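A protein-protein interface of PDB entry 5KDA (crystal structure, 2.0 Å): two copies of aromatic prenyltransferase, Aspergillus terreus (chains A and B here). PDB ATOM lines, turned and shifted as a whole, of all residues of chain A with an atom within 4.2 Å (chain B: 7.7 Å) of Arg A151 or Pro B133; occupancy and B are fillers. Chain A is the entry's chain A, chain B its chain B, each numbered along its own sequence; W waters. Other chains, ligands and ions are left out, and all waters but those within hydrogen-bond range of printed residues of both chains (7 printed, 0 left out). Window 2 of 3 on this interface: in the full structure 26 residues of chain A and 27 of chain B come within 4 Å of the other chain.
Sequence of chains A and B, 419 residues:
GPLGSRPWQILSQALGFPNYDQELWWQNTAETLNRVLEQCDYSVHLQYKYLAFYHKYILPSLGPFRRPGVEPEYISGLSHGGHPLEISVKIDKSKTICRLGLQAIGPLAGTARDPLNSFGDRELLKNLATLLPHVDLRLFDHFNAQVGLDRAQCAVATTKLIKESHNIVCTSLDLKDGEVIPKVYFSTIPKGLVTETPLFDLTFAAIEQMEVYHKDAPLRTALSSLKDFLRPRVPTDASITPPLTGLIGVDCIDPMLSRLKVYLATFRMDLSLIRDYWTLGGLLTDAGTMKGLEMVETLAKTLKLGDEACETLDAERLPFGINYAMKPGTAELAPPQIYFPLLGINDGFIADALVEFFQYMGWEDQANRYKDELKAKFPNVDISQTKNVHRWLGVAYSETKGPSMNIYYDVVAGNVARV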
ATOM      1  N   ALA A 112      26.101 -18.530  18.522  1.00  0.00           N
ATOM      2  CA  ALA A 112      25.472 -17.573  17.535  1.00  0.00           C
ATOM      3  C   ALA A 112      25.582 -17.987  16.085  1.00  0.00           C
ATOM      4  O   ALA A 112      24.650 -17.781  15.300  1.00  0.00           O
ATOM      5  CB  ALA A 112      25.947 -16.115  17.704  1.00  0.00           C
ATOM      6  N   ARG A 113      26.661 -18.663  15.733  1.00  0.00           N
ATOM      7  CA  ARG A 113      26.821 -19.055  14.311  1.00  0.00           C
ATOM      8  C   ARG A 113      26.027 -20.301  13.922  1.00  0.00           C
ATOM      9  O   ARG A 113      25.970 -20.594  12.749  1.00  0.00           O
ATOM     10  CB  ARG A 113      28.268 -19.215  13.929  1.00  0.00           C
ATOM     11  CG  ARG A 113      29.109 -17.933  13.999  1.00  0.00           C
ATOM     12  CD  ARG A 113      30.615 -18.266  13.970  1.00  0.00           C
ATOM     13  NE  ARG A 113      31.426 -17.073  14.122  1.00  0.00           N
ATOM     14  CZ  ARG A 113      31.729 -16.213  13.173  1.00  0.00           C
ATOM     15  NH1 ARG A 113      31.400 -16.431  11.924  1.00  0.00           N
ATOM     16  NH2 ARG A 113      32.445 -15.123  13.478  1.00  0.00           N
ATOM     17  N   ASP A 150      16.731 -20.019   8.937  1.00  0.00           N
ATOM     18  CA  ASP A 150      17.964 -19.240   8.789  1.00  0.00           C
ATOM     19  C   ASP A 150      18.548 -18.866  10.180  1.00  0.00           C
ATOM     20  O   ASP A 150      17.927 -19.161  11.211  1.00  0.00           O
ATOM     21  CB  ASP A 150      17.686 -18.061   7.877  1.00  0.00           C
ATOM     22  CG  ASP A 150      16.971 -16.918   8.554  1.00  0.00           C
ATOM     23  OD1 ASP A 150      16.917 -16.815   9.802  1.00  0.00           O
ATOM     24  OD2 ASP A 150      16.525 -16.083   7.787  1.00  0.00           O
ATOM     25  N   ARG A 151      19.715 -18.213  10.234  1.00  0.00           N
ATOM     26  CA  ARG A 151      20.353 -17.993  11.540  1.00  0.00           C
ATOM     27  C   ARG A 151      19.551 -17.108  12.436  1.00  0.00           C
ATOM     28  O   ARG A 151      19.372 -17.472  13.554  1.00  0.00           O
ATOM     29  CB  ARG A 151      21.773 -17.386  11.443  1.00  0.00           C
ATOM     30  CG  ARG A 151      22.419 -17.093  12.778  1.00  0.00           C
ATOM     31  CD  ARG A 151      23.785 -16.428  12.595  1.00  0.00           C
ATOM     32  NE  ARG A 151      24.706 -17.157  11.706  1.00  0.00           N
ATOM     33  CZ  ARG A 151      25.966 -16.755  11.449  1.00  0.00           C
ATOM     34  NH1 ARG A 151      26.435 -15.693  12.046  1.00  0.00           N
ATOM     35  NH2 ARG A 151      26.765 -17.427  10.611  1.00  0.00           N
ATOM     36  N   ALA A 152      19.150 -15.925  11.971  1.00  0.00           N
ATOM     37  CA  ALA A 152      18.235 -15.025  12.733  1.00  0.00           C
ATOM     38  C   ALA A 152      16.974 -15.741  13.300  1.00  0.00           C
ATOM     39  O   ALA A 152      16.662 -15.531  14.471  1.00  0.00           O
ATOM     40  CB  ALA A 152      17.759 -13.868  11.822  1.00  0.00           C
ATOM     41  N   GLN A 153      16.257 -16.536  12.479  1.00  0.00           N
ATOM     42  CA  GLN A 153      15.151 -17.387  12.945  1.00  0.00           C
ATOM     43  C   GLN A 153      15.579 -18.441  13.959  1.00  0.00           C
ATOM     44  O   GLN A 153      14.897 -18.624  14.971  1.00  0.00           O
ATOM     45  CB  GLN A 153      14.396 -18.098  11.791  1.00  0.00           C
ATOM     46  CG  GLN A 153      13.699 -17.167  10.773  1.00  0.00           C
ATOM     47  CD  GLN A 153      13.164 -17.991   9.601  1.00  0.00           C
ATOM     48  OE1 GLN A 153      13.926 -18.755   8.991  1.00  0.00           O
ATOM     49  NE2 GLN A 153      11.817 -17.885   9.320  1.00  0.00           N
ATOM     50  N   CYS A 154      16.708 -19.106  13.745  1.00  0.00           N
ATOM     51  CA  CYS A 154      17.223 -20.016  14.799  1.00  0.00           C
ATOM     52  C   CYS A 154      17.510 -19.277  16.110  1.00  0.00           C
ATOM     53  O   CYS A 154      17.291 -19.815  17.197  1.00  0.00           O
ATOM     54  CB  CYS A 154      18.513 -20.735  14.361  1.00  0.00           C
ATOM     55  SG  CYS A 154      18.372 -21.915  13.006  1.00  0.00           S
ATOM     56  N   ALA A 155      18.051 -18.076  16.033  1.00  0.00           N
ATOM     57  CA  ALA A 155      18.302 -17.338  17.295  1.00  0.00           C
ATOM     58  C   ALA A 155      16.973 -17.046  17.992  1.00  0.00           C
ATOM     59  O   ALA A 155      16.827 -17.294  19.205  1.00  0.00           O
ATOM     60  CB  ALA A 155      19.064 -16.068  17.056  1.00  0.00           C
ATOM     61  N   LYS B 126      27.641 -24.773   3.331  1.00  0.00           N
ATOM     62  CA  LYS B 126      27.570 -25.003   4.764  1.00  0.00           C
ATOM     63  C   LYS B 126      28.641 -24.175   5.515  1.00  0.00           C
ATOM     64  O   LYS B 126      28.344 -23.493   6.513  1.00  0.00           O
ATOM     65  CB  LYS B 126      27.730 -26.489   5.111  1.00  0.00           C
ATOM     66  CG  LYS B 126      28.070 -26.733   6.592  1.00  0.00           C
ATOM     67  CD  LYS B 126      28.837 -28.009   6.805  1.00  0.00           C
ATOM     68  CE  LYS B 126      30.313 -27.861   6.482  1.00  0.00           C
ATOM     69  NZ  LYS B 126      31.020 -29.171   6.545  1.00  0.00           N
ATOM     70  N   ASN B 127      29.876 -24.230   5.037  1.00  0.00           N
ATOM     71  CA  ASN B 127      30.938 -23.398   5.650  1.00  0.00           C
ATOM     72  C   ASN B 127      30.632 -21.920   5.562  1.00  0.00           C
ATOM     73  O   ASN B 127      30.923 -21.216   6.503  1.00  0.00           O
ATOM     74  CB  ASN B 127      32.305 -23.650   5.078  1.00  0.00           C
ATOM     75  CG  ASN B 127      32.788 -25.043   5.345  1.00  0.00           C
ATOM     76  OD1 ASN B 127      32.483 -25.605   6.366  1.00  0.00           O
ATOM     77  ND2 ASN B 127      33.518 -25.603   4.408  1.00  0.00           N
ATOM     78  N   LEU B 128      29.993 -21.472   4.497  1.00  0.00           N
ATOM     79  CA  LEU B 128      29.604 -20.088   4.386  1.00  0.00           C
ATOM     80  C   LEU B 128      28.487 -19.690   5.324  1.00  0.00           C
ATOM     81  O   LEU B 128      28.413 -18.531   5.723  1.00  0.00           O
ATOM     82  CB  LEU B 128      29.212 -19.705   2.943  1.00  0.00           C
ATOM     83  CG  LEU B 128      30.257 -20.002   1.880  1.00  0.00           C
ATOM     84  CD1 LEU B 128      29.863 -19.432   0.529  1.00  0.00           C
ATOM     85  CD2 LEU B 128      31.641 -19.542   2.341  1.00  0.00           C
ATOM     86  N   ALA B 129      27.596 -20.626   5.637  1.00  0.00           N
ATOM     87  CA  ALA B 129      26.452 -20.372   6.492  1.00  0.00           C
ATOM     88  C   ALA B 129      26.884 -20.194   7.899  1.00  0.00           C
ATOM     89  O   ALA B 129      26.216 -19.530   8.625  1.00  0.00           O
ATOM     90  CB  ALA B 129      25.484 -21.556   6.459  1.00  0.00           C
ATOM     91  N   THR B 130      27.994 -20.792   8.315  1.00  0.00           N
ATOM     92  CA  THR B 130      28.534 -20.471   9.624  1.00  0.00           C
ATOM     93  C   THR B 130      29.509 -19.261   9.600  1.00  0.00           C
ATOM     94  O   THR B 130      29.770 -18.703  10.634  1.00  0.00           O
ATOM     95  CB  THR B 130      29.294 -21.659  10.262  1.00  0.00           C
ATOM     96  OG1 THR B 130      30.325 -21.995   9.401  1.00  0.00           O
ATOM     97  CG2 THR B 130      28.414 -22.874  10.509  1.00  0.00           C
ATOM     98  N   LEU B 131      30.084 -18.926   8.449  1.00  0.00           N
ATOM     99  CA  LEU B 131      30.866 -17.698   8.283  1.00  0.00           C
ATOM    100  C   LEU B 131      30.038 -16.368   8.252  1.00  0.00           C
ATOM    101  O   LEU B 131      30.389 -15.379   8.880  1.00  0.00           O
ATOM    102  CB  LEU B 131      31.622 -17.799   6.956  1.00  0.00           C
ATOM    103  CG  LEU B 131      32.561 -16.649   6.555  1.00  0.00           C
ATOM    104  CD1 LEU B 131      33.609 -16.464   7.616  1.00  0.00           C
ATOM    105  CD2 LEU B 131      33.138 -16.777   5.133  1.00  0.00           C
ATOM    106  N   LEU B 132      28.993 -16.368   7.430  1.00  0.00           N
ATOM    107  CA  LEU B 132      28.231 -15.216   7.011  1.00  0.00           C
ATOM    108  C   LEU B 132      26.759 -15.224   7.549  1.00  0.00           C
ATOM    109  O   LEU B 132      25.978 -16.110   7.216  1.00  0.00           O
ATOM    110  CB  LEU B 132      28.205 -15.221   5.503  1.00  0.00           C
ATOM    111  CG  LEU B 132      29.515 -15.265   4.720  1.00  0.00           C
ATOM    112  CD1 LEU B 132      29.272 -15.790   3.308  1.00  0.00           C
ATOM    113  CD2 LEU B 132      30.151 -13.890   4.736  1.00  0.00           C
ATOM    114  N   PRO B 133      26.339 -14.175   8.283  1.00  0.00           N
ATOM    115  CA  PRO B 133      24.950 -14.169   8.836  1.00  0.00           C
ATOM    116  C   PRO B 133      23.791 -14.248   7.828  1.00  0.00           C
ATOM    117  O   PRO B 133      22.723 -14.763   8.178  1.00  0.00           O
ATOM    118  CB  PRO B 133      24.861 -12.837   9.603  1.00  0.00           C
ATOM    119  CG  PRO B 133      25.985 -11.983   9.081  1.00  0.00           C
ATOM    120  CD  PRO B 133      27.080 -12.932   8.616  1.00  0.00           C
ATOM    121  N   HIS B 134      23.944 -13.744   6.612  1.00  0.00           N
ATOM    122  CA  HIS B 134      22.750 -13.653   5.739  1.00  0.00           C
ATOM    123  C   HIS B 134      22.688 -14.724   4.688  1.00  0.00           C
ATOM    124  O   HIS B 134      21.942 -14.595   3.714  1.00  0.00           O
ATOM    125  CB  HIS B 134      22.649 -12.261   5.103  1.00  0.00           C
ATOM    126  CG  HIS B 134      22.800 -11.166   6.101  1.00  0.00           C
ATOM    127  ND1 HIS B 134      22.116 -11.165   7.303  1.00  0.00           N
ATOM    128  CD2 HIS B 134      23.606 -10.074   6.122  1.00  0.00           C
ATOM    129  CE1 HIS B 134      22.484 -10.113   8.013  1.00  0.00           C
ATOM    130  NE2 HIS B 134      23.391  -9.442   7.324  1.00  0.00           N
ATOM    131  N   VAL B 135      23.457 -15.784   4.859  1.00  0.00           N
ATOM    132  CA  VAL B 135      23.475 -16.856   3.889  1.00  0.00           C
ATOM    133  C   VAL B 135      22.320 -17.786   4.264  1.00  0.00           C
ATOM    134  O   VAL B 135      22.134 -18.113   5.426  1.00  0.00           O
ATOM    135  CB  VAL B 135      24.816 -17.619   3.881  1.00  0.00           C
ATOM    136  CG1 VAL B 135      24.711 -18.818   3.002  1.00  0.00           C
ATOM    137  CG2 VAL B 135      25.879 -16.722   3.346  1.00  0.00           C
ATOM    138  N   ASP B 136      21.525 -18.172   3.284  1.00  0.00           N
ATOM    139  CA  ASP B 136      20.339 -18.996   3.532  1.00  0.00           C
ATOM    140  C   ASP B 136      20.391 -20.132   2.524  1.00  0.00           C
ATOM    141  O   ASP B 136      20.538 -19.873   1.350  1.00  0.00           O
ATOM    142  CB  ASP B 136      19.121 -18.128   3.283  1.00  0.00           C
ATOM    143  CG  ASP B 136      17.821 -18.760   3.747  1.00  0.00           C
ATOM    144  OD1 ASP B 136      17.605 -19.988   3.645  1.00  0.00           O
ATOM    145  OD2 ASP B 136      16.957 -17.979   4.150  1.00  0.00           O
ATOM    146  N   ARG B 138      17.978 -22.528   1.985  1.00  0.00           N
ATOM    147  CA  ARG B 138      16.711 -23.229   1.806  1.00  0.00           C
ATOM    148  C   ARG B 138      16.353 -23.414   0.353  1.00  0.00           C
ATOM    149  O   ARG B 138      15.818 -24.491   0.001  1.00  0.00           O
ATOM    150  CB  ARG B 138      15.626 -22.577   2.612  1.00  0.00           C
ATOM    151  CG  ARG B 138      15.774 -22.927   4.102  1.00  0.00           C
ATOM    152  CD  ARG B 138      14.874 -22.135   5.029  1.00  0.00           C
ATOM    153  NE  ARG B 138      15.070 -20.689   4.976  1.00  0.00           N
ATOM    154  CZ  ARG B 138      14.484 -19.828   5.794  1.00  0.00           C
ATOM    155  NH1 ARG B 138      13.642 -20.265   6.721  1.00  0.00           N
ATOM    156  NH2 ARG B 138      14.731 -18.536   5.695  1.00  0.00           N
ATOM    157  N   GLU B 179      30.563  -7.606   1.252  1.00  0.00           N
ATOM    158  CA  GLU B 179      29.982  -8.909   1.623  1.00  0.00           C
ATOM    159  C   GLU B 179      30.318  -9.949   0.562  1.00  0.00           C
ATOM    160  O   GLU B 179      30.781  -9.609  -0.512  1.00  0.00           O
ATOM    161  CB  GLU B 179      28.444  -8.818   1.780  1.00  0.00           C
ATOM    162  CG  GLU B 179      27.963  -8.182   3.097  1.00  0.00           C
ATOM    163  CD  GLU B 179      28.523  -8.892   4.349  1.00  0.00           C
ATOM    164  OE1 GLU B 179      28.798 -10.123   4.331  1.00  0.00           O
ATOM    165  OE2 GLU B 179      28.728  -8.210   5.357  1.00  0.00           O
HETATM  166  O   HOH W   1      19.948 -14.976   9.392  1.00  0.00           O
HETATM  167  O   HOH W   2      10.372 -19.451   7.603  1.00  0.00           O
HETATM  168  O   HOH W   3      24.120 -20.050  10.970  1.00  0.00           O
HETATM  169  O   HOH W   4      21.076 -17.236   8.022  1.00  0.00           O
HETATM  170  O   HOH W   5      13.593 -16.212   6.568  1.00  0.00           O
HETATM  171  O   HOH W   6      32.750 -14.158  10.878  1.00  0.00           O
HETATM  172  O   HOH W   7      28.637 -14.581  10.990  1.00  0.00           O
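Asp A150 touches Asp B136 (CB to OD2, 3.8 Å). O of Leu B132 touches NH2 of Arg A151, at 3.7 Å. Arg A151 touches Pro B133.
OD2 of Asp B136 is in salt-bridge range of NH2 of Arg B138 (2.8 Å). O of Asn B127 sits at hydrogen-bond distance from OG1 of Thr B130 (3.1 Å). The side-chain carboxylate of Asp A150 sits at hydrogen-bond distance from the backbone NH of Ala A152, 3.2 Å away. The side-chain carboxylate of Asp A150 sits at hydrogen-bond distance from the backbone NH of Gln A153 (2.8 Å). The backbone carbonyl oxygen (O) of Asp A150 is in hydrogen-bond range of the side-chain sulfur (SG) of Cys A154, 3.3 Å away.
The guanidinium group of Arg A113 is in hydrogen-bond range of the backbone carbonyl oxygen of Thr B130 (3.1 Å). OE1 of Gln A153 is in hydrogen-bond range of NH1 of Arg B138, at 2.7 Å. NH1 of Arg A113 sits at hydrogen-bond distance from O of Leu B131 (3.4 Å). O of Ala B129 is in hydrogen-bond range of NH2 of Arg A151. NH2 of Arg A151 lies within hydrogen-bond range of O of Thr B130, 3.3 Å away. The guanidinium group (NH2) of Arg B138 is in salt-bridge range of the side-chain carboxylate (OD2) of Asp A150 (3.7 Å).
Pro B133 touches just one residue of chain A: Arg A151 (3.8 Å). Printed residues of chain B within 4 Å of Gln A153: Arg B138. Of the printed residues of chain A, Arg B138 touches Asp A150 and Gln A153. Ala A152 touches none of the printed residues of chain B. Val B135 touches none of the printed residues of chain A. The nearest residue of chain B that does not touch Arg A151 is Leu B131 (4.2 Å).
No position is printed for both chains. Of the 9 pairs that touch across the chains among the printed residues, none has its exchanged pair printed and touching as well.
Printed residues of chain B that touch a printed residue of chain A: Ala B129, Thr B130, Leu B131, Leu B132, Pro B133, Asp B136 and Arg B138. Along chain B the printed residues that touch a printed residue of chain A span positions 129 to 138. Among the printed residues, Asp or Glu carboxylates within 4 Å of a Lys or Arg side-chain nitrogen of the other chain: Asp A150 with Arg B138.
Water W3 lies within hydrogen-bond range of O of Arg A113 (2.6 Å), NE of Arg A151 (3.0 Å) and O of Ala B129 (3.2 Å). Water W7 lies within hydrogen-bond range of NH1 of Arg A151 (2.7 Å), O of Leu B131 (2.9 Å) and NH1 of Arg A113 (3.5 Å). Water W5 lies within hydrogen-bond range of the guanidinium group (NH2) of Arg B138 (2.7 Å) and the side-chain carboxylate (OD2) of Asp A150 (3.2 Å). Water W2 bridges the side-chain amide nitrogen of Gln A153 (2.7 Å) and the guanidinium group of Arg B138 (3.5 Å). Water W6 lies within hydrogen-bond range of NH2 of Arg A113 and O of Leu B131. Water W1 lies within hydrogen-bond range of the backbone NH of Ala A152 (2.9 Å), the backbone carbonyl oxygen of Pro B133 (3.0 Å) and the backbone NH of Arg A151 (3.4 Å).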
